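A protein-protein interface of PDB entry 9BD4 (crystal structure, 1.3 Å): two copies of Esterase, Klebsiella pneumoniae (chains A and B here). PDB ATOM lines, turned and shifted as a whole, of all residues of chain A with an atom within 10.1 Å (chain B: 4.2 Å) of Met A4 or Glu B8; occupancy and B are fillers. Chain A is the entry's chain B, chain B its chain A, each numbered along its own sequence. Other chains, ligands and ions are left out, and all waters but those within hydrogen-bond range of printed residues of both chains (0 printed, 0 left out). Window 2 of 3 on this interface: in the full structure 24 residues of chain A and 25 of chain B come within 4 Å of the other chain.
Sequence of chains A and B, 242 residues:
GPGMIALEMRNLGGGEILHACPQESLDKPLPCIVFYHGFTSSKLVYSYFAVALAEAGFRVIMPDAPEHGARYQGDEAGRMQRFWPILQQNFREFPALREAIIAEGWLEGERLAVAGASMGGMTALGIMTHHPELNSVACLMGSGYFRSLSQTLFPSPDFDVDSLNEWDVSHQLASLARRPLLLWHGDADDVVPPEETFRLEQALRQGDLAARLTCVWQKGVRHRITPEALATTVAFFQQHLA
Hydrophobic or aromatic side chains of chain A within 4 Å of the printed part of chain B: Met A4 and Ile A5.
Of the printed residues of chain B, Met A4 touches Ala B6, Leu B7, Glu B8 and Leu B26. Glu B8 touches just one residue of chain A: Met A4 (3.4 Å). Of chain A, only Met A4, Ile A5 and Gln A23 come within 4 Å of Ala B6. No residue of chain A comes within 4 Å of Leu B18. No residue of chain A comes within 4 Å of His B19. Printed residues of chain A within 4 Å of Leu B7: Met A4 (3.5 Å) and Ile A5 (2.8 Å). Printed residues of chain B within 4 Å of Ile A5: Ala B6 (3.4 Å) and Leu B7 (2.8 Å). Of the printed residues of chain B, Gln A23 touches Ala B6 (3.6 Å). Of the printed residues of chain A, Leu B26 touches Met A4 (3.7 Å). The nearest printed residue of chain A that does not touch Leu B26 is Gln A23 (5.5 Å).
Met A4 touches Ala B6. Leu B7 touches Met A4 (O to CA, 3.5 Å). OE2 of Glu B8 touches CE of Met A4, 3.4 Å away. Leu B26 touches Met A4. Ile A5 touches Ala B6. Ala B6 touches Gln A23.
Positions printed for both chains: 6, 7 and 26. Of the 7 pairs that touch across the chains among the printed residues, none has its exchanged pair printed and touching as well.
NH2 of Arg B10 lies within salt-bridge range of OE1 of Glu B8 (2.7 Å). The side-chain amide nitrogen (NE2) of Gln A23 is in hydrogen-bond range of the backbone carbonyl oxygen (O) of Ile A5 (3.2 Å). O of Met A4 sits at hydrogen-bond distance from N of Gln A23 (3.0 Å). The backbone carbonyl oxygen (O) of Glu B8 sits at hydrogen-bond distance from the backbone NH (N) of His B19 (2.9 Å).
O of Leu B7 lies within hydrogen-bond range of N of Ile A5 (2.8 Å).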
ATOM      1  N   MET A   4       8.443  -9.494  30.938  1.00  0.00           N
ATOM      2  CA  MET A   4       8.685  -8.071  31.177  1.00  0.00           C
ATOM      3  C   MET A   4      10.143  -7.733  30.863  1.00  0.00           C
ATOM      4  O   MET A   4      11.074  -8.441  31.294  1.00  0.00           O
ATOM      5  CB  MET A   4       8.400  -7.736  32.640  1.00  0.00           C
ATOM      6  CG  MET A   4       8.819  -6.337  33.061  1.00  0.00           C
ATOM      7  SD  MET A   4       7.840  -5.611  34.401  1.00  0.00           S
ATOM      8  CE  MET A   4       6.652  -4.625  33.497  1.00  0.00           C
ATOM      9  N   ILE A   5      10.361  -6.648  30.132  1.00  0.00           N
ATOM     10  CA  ILE A   5      11.712  -6.246  29.775  1.00  0.00           C
ATOM     11  C   ILE A   5      12.037  -4.899  30.402  1.00  0.00           C
ATOM     12  O   ILE A   5      11.155  -4.107  30.750  1.00  0.00           O
ATOM     13  CB  ILE A   5      11.990  -6.248  28.254  1.00  0.00           C
ATOM     14  CG1 ILE A   5      11.122  -5.213  27.544  1.00  0.00           C
ATOM     15  CG2 ILE A   5      11.797  -7.654  27.662  1.00  0.00           C
ATOM     16  CD1 ILE A   5      11.548  -4.973  26.094  1.00  0.00           C
ATOM     17  N   ALA A   6      13.338  -4.668  30.568  1.00  0.00           N
ATOM     18  CA  ALA A   6      13.879  -3.418  31.071  1.00  0.00           C
ATOM     19  C   ALA A   6      14.636  -2.751  29.935  1.00  0.00           C
ATOM     20  O   ALA A   6      15.298  -3.425  29.142  1.00  0.00           O
ATOM     21  CB  ALA A   6      14.854  -3.671  32.233  1.00  0.00           C
ATOM     22  N   LEU A   7      14.547  -1.428  29.859  1.00  0.00           N
ATOM     23  CA  LEU A   7      15.284  -0.690  28.846  1.00  0.00           C
ATOM     24  C   LEU A   7      15.809   0.592  29.472  1.00  0.00           C
ATOM     25  O   LEU A   7      15.089   1.283  30.196  1.00  0.00           O
ATOM     26  CB  LEU A   7      14.397  -0.402  27.619  1.00  0.00           C
ATOM     27  CG  LEU A   7      15.003   0.235  26.369  1.00  0.00           C
ATOM     28  CD1 LEU A   7      14.160  -0.121  25.155  1.00  0.00           C
ATOM     29  CD2 LEU A   7      15.110   1.748  26.500  1.00  0.00           C
ATOM     30  N   ALA A  20      18.591  -3.062  26.321  1.00  0.00           N
ATOM     31  CA  ALA A  20      17.354  -3.741  26.687  1.00  0.00           C
ATOM     32  C   ALA A  20      17.647  -5.199  27.008  1.00  0.00           C
ATOM     33  O   ALA A  20      18.512  -5.821  26.385  1.00  0.00           O
ATOM     34  CB  ALA A  20      16.310  -3.668  25.568  1.00  0.00           C
ATOM     35  N   CYS A  21      16.934  -5.739  27.994  1.00  0.00           N
ATOM     36  CA  CYS A  21      17.104  -7.139  28.370  1.00  0.00           C
ATOM     37  C   CYS A  21      15.907  -7.561  29.210  1.00  0.00           C
ATOM     38  O   CYS A  21      15.168  -6.710  29.722  1.00  0.00           O
ATOM     39  CB  CYS A  21      18.420  -7.351  29.151  1.00  0.00           C
ATOM     40  SG  CYS A  21      18.447  -6.581  30.784  1.00  0.00           S
ATOM     41  N   PRO A  22      15.698  -8.866  29.390  1.00  0.00           N
ATOM     42  CA  PRO A  22      14.662  -9.312  30.331  1.00  0.00           C
ATOM     43  C   PRO A  22      14.923  -8.746  31.724  1.00  0.00           C
ATOM     44  O   PRO A  22      16.063  -8.708  32.193  1.00  0.00           O
ATOM     45  CB  PRO A  22      14.801 -10.841  30.306  1.00  0.00           C
ATOM     46  CG  PRO A  22      15.440 -11.137  28.966  1.00  0.00           C
ATOM     47  CD  PRO A  22      16.367 -10.001  28.723  1.00  0.00           C
ATOM     48  N   GLN A  23      13.854  -8.296  32.390  1.00  0.00           N
ATOM     49  CA  GLN A  23      14.011  -7.717  33.726  1.00  0.00           C
ATOM     50  C   GLN A  23      14.681  -8.680  34.695  1.00  0.00           C
ATOM     51  O   GLN A  23      15.528  -8.272  35.496  1.00  0.00           O
ATOM     52  CB  GLN A  23      12.665  -7.270  34.288  1.00  0.00           C
ATOM     53  CG  GLN A  23      12.086  -6.086  33.578  1.00  0.00           C
ATOM     54  CD  GLN A  23      12.212  -4.825  34.400  1.00  0.00           C
ATOM     55  OE1 GLN A  23      12.737  -4.851  35.516  1.00  0.00           O
ATOM     56  NE2 GLN A  23      11.718  -3.713  33.863  1.00  0.00           N
ATOM     57  N   GLU A  24      14.318  -9.960  34.637  1.00  0.00           N
ATOM     58  CA  GLU A  24      14.880 -10.920  35.575  1.00  0.00           C
ATOM     59  C   GLU A  24      16.373 -11.142  35.365  1.00  0.00           C
ATOM     60  O   GLU A  24      17.006 -11.790  36.204  1.00  0.00           O
ATOM     61  CB  GLU A  24      14.162 -12.261  35.434  1.00  0.00           C
ATOM     62  CG  GLU A  24      14.487 -12.986  34.135  1.00  0.00           C
ATOM     63  CD  GLU A  24      13.382 -12.890  33.105  1.00  0.00           C
ATOM     64  OE1 GLU A  24      12.673 -11.856  33.083  1.00  0.00           O
ATOM     65  OE2 GLU A  24      13.228 -13.848  32.315  1.00  0.00           O
ATOM     66  N   SER A  25      16.947 -10.633  34.276  1.00  0.00           N
ATOM     67  CA  SER A  25      18.340 -10.896  33.930  1.00  0.00           C
ATOM     68  C   SER A  25      19.219  -9.653  33.977  1.00  0.00           C
ATOM     69  O   SER A  25      20.337  -9.687  33.450  1.00  0.00           O
ATOM     70  CB  SER A  25      18.436 -11.548  32.544  1.00  0.00           C
ATOM     71  OG  SER A  25      17.757 -12.788  32.515  1.00  0.00           O
ATOM     72  N   LEU A  26      18.757  -8.566  34.603  1.00  0.00           N
ATOM     73  CA  LEU A  26      19.535  -7.328  34.632  1.00  0.00           C
ATOM     74  C   LEU A  26      20.928  -7.516  35.228  1.00  0.00           C
ATOM     75  O   LEU A  26      21.870  -6.824  34.823  1.00  0.00           O
ATOM     76  CB  LEU A  26      18.779  -6.260  35.423  1.00  0.00           C
ATOM     77  CG  LEU A  26      17.814  -5.405  34.606  1.00  0.00           C
ATOM     78  CD1 LEU A  26      16.870  -4.657  35.531  1.00  0.00           C
ATOM     79  CD2 LEU A  26      18.573  -4.433  33.705  1.00  0.00           C
ATOM     80  N   LEU A  30      24.313 -12.407  29.377  1.00  0.00           N
ATOM     81  CA  LEU A  30      23.361 -12.974  28.435  1.00  0.00           C
ATOM     82  C   LEU A  30      24.001 -13.041  27.059  1.00  0.00           C
ATOM     83  O   LEU A  30      24.977 -12.332  26.786  1.00  0.00           O
ATOM     84  CB  LEU A  30      22.108 -12.092  28.330  1.00  0.00           C
ATOM     85  CG  LEU A  30      21.089 -12.183  29.469  1.00  0.00           C
ATOM     86  CD1 LEU A  30      20.005 -11.136  29.252  1.00  0.00           C
ATOM     87  CD2 LEU A  30      20.466 -13.556  29.561  1.00  0.00           C
ATOM     88  N   ALA A  50      15.184  -3.726  19.779  1.00  0.00           N
ATOM     89  CA  ALA A  50      15.583  -4.064  21.140  1.00  0.00           C
ATOM     90  C   ALA A  50      14.414  -4.633  21.933  1.00  0.00           C
ATOM     91  O   ALA A  50      14.588  -5.594  22.689  1.00  0.00           O
ATOM     92  CB  ALA A  50      16.187  -2.842  21.836  1.00  0.00           C
ATOM     93  N   VAL A  51      13.217  -4.059  21.779  1.00  0.00           N
ATOM     94  CA  VAL A  51      12.032  -4.607  22.432  1.00  0.00           C
ATOM     95  C   VAL A  51      11.785  -6.041  21.977  1.00  0.00           C
ATOM     96  O   VAL A  51      11.625  -6.955  22.797  1.00  0.00           O
ATOM     97  CB  VAL A  51      10.809  -3.710  22.170  1.00  0.00           C
ATOM     98  CG1 VAL A  51       9.560  -4.332  22.770  1.00  0.00           C
ATOM     99  CG2 VAL A  51      11.038  -2.296  22.748  1.00  0.00           C
ATOM    100  N   LEU A  53      13.728  -8.299  20.457  1.00  0.00           N
ATOM    101  CA  LEU A  53      14.753  -9.297  20.762  1.00  0.00           C
ATOM    102  C   LEU A  53      14.892  -9.527  22.265  1.00  0.00           C
ATOM    103  O   LEU A  53      15.161 -10.659  22.689  1.00  0.00           O
ATOM    104  CB  LEU A  53      16.085  -8.899  20.117  1.00  0.00           C
ATOM    105  CG  LEU A  53      16.111  -9.038  18.590  1.00  0.00           C
ATOM    106  CD1 LEU A  53      17.209  -8.180  17.963  1.00  0.00           C
ATOM    107  CD2 LEU A  53      16.276 -10.504  18.191  1.00  0.00           C
ATOM    108  N   ALA A  54      14.684  -8.490  23.089  1.00  0.00           N
ATOM    109  CA  ALA A  54      14.687  -8.705  24.536  1.00  0.00           C
ATOM    110  C   ALA A  54      13.504  -9.559  24.970  1.00  0.00           C
ATOM    111  O   ALA A  54      13.624 -10.374  25.889  1.00  0.00           O
ATOM    112  CB  ALA A  54      14.689  -7.373  25.286  1.00  0.00           C
ATOM    113  N   GLU A  55      12.343  -9.388  24.325  1.00  0.00           N
ATOM    114  CA  GLU A  55      11.205 -10.243  24.641  1.00  0.00           C
ATOM    115  C   GLU A  55      11.504 -11.703  24.325  1.00  0.00           C
ATOM    116  O   GLU A  55      10.916 -12.602  24.936  1.00  0.00           O
ATOM    117  CB  GLU A  55       9.955  -9.760  23.901  1.00  0.00           C
ATOM    118  CG  GLU A  55       9.316  -8.510  24.500  1.00  0.00           C
ATOM    119  CD  GLU A  55       8.538  -8.783  25.782  1.00  0.00           C
ATOM    120  OE1 GLU A  55       8.455  -9.958  26.195  1.00  0.00           O
ATOM    121  OE2 GLU A  55       8.006  -7.818  26.380  1.00  0.00           O
ATOM    122  N   ALA A  56      12.426 -11.956  23.399  1.00  0.00           N
ATOM    123  CA  ALA A  56      12.849 -13.307  23.063  1.00  0.00           C
ATOM    124  C   ALA A  56      13.958 -13.820  23.972  1.00  0.00           C
ATOM    125  O   ALA A  56      14.428 -14.947  23.775  1.00  0.00           O
ATOM    126  CB  ALA A  56      13.313 -13.358  21.604  1.00  0.00           C
ATOM    127  N   GLY A  57      14.389 -13.025  24.950  1.00  0.00           N
ATOM    128  CA  GLY A  57      15.364 -13.451  25.935  1.00  0.00           C
ATOM    129  C   GLY A  57      16.773 -12.926  25.732  1.00  0.00           C
ATOM    130  O   GLY A  57      17.662 -13.275  26.517  1.00  0.00           O
ATOM    131  N   PHE A  58      17.011 -12.097  24.725  1.00  0.00           N
ATOM    132  CA  PHE A  58      18.353 -11.594  24.459  1.00  0.00           C
ATOM    133  C   PHE A  58      18.601 -10.265  25.170  1.00  0.00           C
ATOM    134  O   PHE A  58      17.673  -9.549  25.547  1.00  0.00           O
ATOM    135  CB  PHE A  58      18.572 -11.383  22.954  1.00  0.00           C
ATOM    136  CG  PHE A  58      18.446 -12.642  22.138  1.00  0.00           C
ATOM    137  CD1 PHE A  58      19.425 -13.613  22.197  1.00  0.00           C
ATOM    138  CD2 PHE A  58      17.357 -12.847  21.306  1.00  0.00           C
ATOM    139  CE1 PHE A  58      19.317 -14.778  21.450  1.00  0.00           C
ATOM    140  CE2 PHE A  58      17.255 -14.011  20.548  1.00  0.00           C
ATOM    141  CZ  PHE A  58      18.235 -14.975  20.628  1.00  0.00           C
ATOM    142  N   ALA B   6      10.059   0.060  31.967  1.00  0.00           N
ATOM    143  CA  ALA B   6       9.579  -1.307  31.910  1.00  0.00           C
ATOM    144  C   ALA B   6       8.627  -1.417  30.736  1.00  0.00           C
ATOM    145  O   ALA B   6       7.856  -0.490  30.463  1.00  0.00           O
ATOM    146  CB  ALA B   6       8.805  -1.652  33.186  1.00  0.00           C
ATOM    147  N   LEU B   7       8.701  -2.531  30.017  1.00  0.00           N
ATOM    148  CA  LEU B   7       7.734  -2.811  28.969  1.00  0.00           C
ATOM    149  C   LEU B   7       7.270  -4.244  29.122  1.00  0.00           C
ATOM    150  O   LEU B   7       8.049  -5.121  29.501  1.00  0.00           O
ATOM    151  CB  LEU B   7       8.312  -2.642  27.563  1.00  0.00           C
ATOM    152  CG  LEU B   7       8.905  -1.297  27.171  1.00  0.00           C
ATOM    153  CD1 LEU B   7      10.406  -1.296  27.429  1.00  0.00           C
ATOM    154  CD2 LEU B   7       8.583  -0.960  25.721  1.00  0.00           C
ATOM    155  N   GLU B   8       5.997  -4.479  28.819  1.00  0.00           N
ATOM    156  CA  GLU B   8       5.442  -5.817  28.922  1.00  0.00           C
ATOM    157  C   GLU B   8       4.301  -5.985  27.933  1.00  0.00           C
ATOM    158  O   GLU B   8       3.605  -5.022  27.593  1.00  0.00           O
ATOM    159  CB  GLU B   8       4.943  -6.080  30.346  1.00  0.00           C
ATOM    160  CG  GLU B   8       3.840  -5.130  30.770  1.00  0.00           C
ATOM    161  CD  GLU B   8       3.317  -5.401  32.168  1.00  0.00           C
ATOM    162  OE1 GLU B   8       2.421  -4.650  32.614  1.00  0.00           O
ATOM    163  OE2 GLU B   8       3.794  -6.359  32.819  1.00  0.00           O
ATOM    164  N   MET B   9       4.133  -7.213  27.449  1.00  0.00           N
ATOM    165  CA  MET B   9       2.915  -7.611  26.757  1.00  0.00           C
ATOM    166  C   MET B   9       1.944  -8.130  27.809  1.00  0.00           C
ATOM    167  O   MET B   9       2.321  -8.952  28.649  1.00  0.00           O
ATOM    168  CB  MET B   9       3.223  -8.734  25.769  1.00  0.00           C
ATOM    169  CG  MET B   9       4.160  -8.356  24.651  1.00  0.00           C
ATOM    170  SD  MET B   9       3.445  -7.013  23.704  1.00  0.00           S
ATOM    171  CE  MET B   9       4.625  -6.867  22.364  1.00  0.00           C
ATOM    172  N   ARG B  10       0.706  -7.644  27.773  1.00  0.00           N
ATOM    173  CA  ARG B  10      -0.306  -7.994  28.764  1.00  0.00           C
ATOM    174  C   ARG B  10      -1.651  -8.105  28.060  1.00  0.00           C
ATOM    175  O   ARG B  10      -1.902  -7.412  27.075  1.00  0.00           O
ATOM    176  CB  ARG B  10      -0.418  -6.873  29.829  1.00  0.00           C
ATOM    177  CG  ARG B  10      -1.678  -6.964  30.692  1.00  0.00           C
ATOM    178  CD  ARG B  10      -1.707  -6.055  31.885  1.00  0.00           C
ATOM    179  NE  ARG B  10      -0.453  -6.006  32.619  1.00  0.00           N
ATOM    180  CZ  ARG B  10      -0.377  -5.798  33.925  1.00  0.00           C
ATOM    181  NH1 ARG B  10      -1.466  -5.711  34.672  1.00  0.00           N
ATOM    182  NH2 ARG B  10       0.817  -5.675  34.495  1.00  0.00           N
ATOM    183  N   ILE B  17      -2.088  -6.204  24.594  1.00  0.00           N
ATOM    184  CA  ILE B  17      -1.550  -4.860  24.454  1.00  0.00           C
ATOM    185  C   ILE B  17      -0.077  -4.861  24.825  1.00  0.00           C
ATOM    186  O   ILE B  17       0.427  -5.772  25.487  1.00  0.00           O
ATOM    187  CB  ILE B  17      -2.318  -3.824  25.306  1.00  0.00           C
ATOM    188  CG1 ILE B  17      -2.252  -4.182  26.802  1.00  0.00           C
ATOM    189  CG2 ILE B  17      -3.772  -3.719  24.846  1.00  0.00           C
ATOM    190  CD1 ILE B  17      -1.282  -3.349  27.616  1.00  0.00           C
ATOM    191  N   LEU B  18       0.606  -3.807  24.402  1.00  0.00           N
ATOM    192  CA  LEU B  18       1.946  -3.503  24.871  1.00  0.00           C
ATOM    193  C   LEU B  18       1.825  -2.335  25.841  1.00  0.00           C
ATOM    194  O   LEU B  18       1.153  -1.340  25.539  1.00  0.00           O
ATOM    195  CB  LEU B  18       2.865  -3.189  23.685  1.00  0.00           C
ATOM    196  CG  LEU B  18       4.339  -2.893  23.924  1.00  0.00           C
ATOM    197  CD1 LEU B  18       5.102  -3.237  22.654  1.00  0.00           C
ATOM    198  CD2 LEU B  18       4.548  -1.438  24.276  1.00  0.00           C
ATOM    199  N   HIS B  19       2.442  -2.470  27.014  1.00  0.00           N
ATOM    200  CA  HIS B  19       2.416  -1.460  28.071  1.00  0.00           C
ATOM    201  C   HIS B  19       3.849  -1.051  28.375  1.00  0.00           C
ATOM    202  O   HIS B  19       4.705  -1.915  28.588  1.00  0.00           O
ATOM    203  CB  HIS B  19       1.762  -2.056  29.336  1.00  0.00           C
ATOM    204  CG  HIS B  19       1.971  -1.264  30.600  1.00  0.00           C
ATOM    205  ND1 HIS B  19       2.309  -1.863  31.793  1.00  0.00           N
ATOM    206  CD2 HIS B  19       1.833   0.057  30.874  1.00  0.00           C
ATOM    207  CE1 HIS B  19       2.407  -0.946  32.740  1.00  0.00           C
ATOM    208  NE2 HIS B  19       2.126   0.230  32.208  1.00  0.00           N
ATOM    209  N   LEU B  26       5.505   1.518  38.155  1.00  0.00           N
ATOM    210  CA  LEU B  26       4.683   0.361  37.807  1.00  0.00           C
ATOM    211  C   LEU B  26       3.448   0.229  38.689  1.00  0.00           C
ATOM    212  O   LEU B  26       2.413  -0.269  38.234  1.00  0.00           O
ATOM    213  CB  LEU B  26       5.517  -0.919  37.899  1.00  0.00           C
ATOM    214  CG  LEU B  26       6.337  -1.246  36.652  1.00  0.00           C
ATOM    215  CD1 LEU B  26       7.408  -2.271  36.996  1.00  0.00           C
ATOM    216  CD2 LEU B  26       5.429  -1.749  35.534  1.00  0.00           C
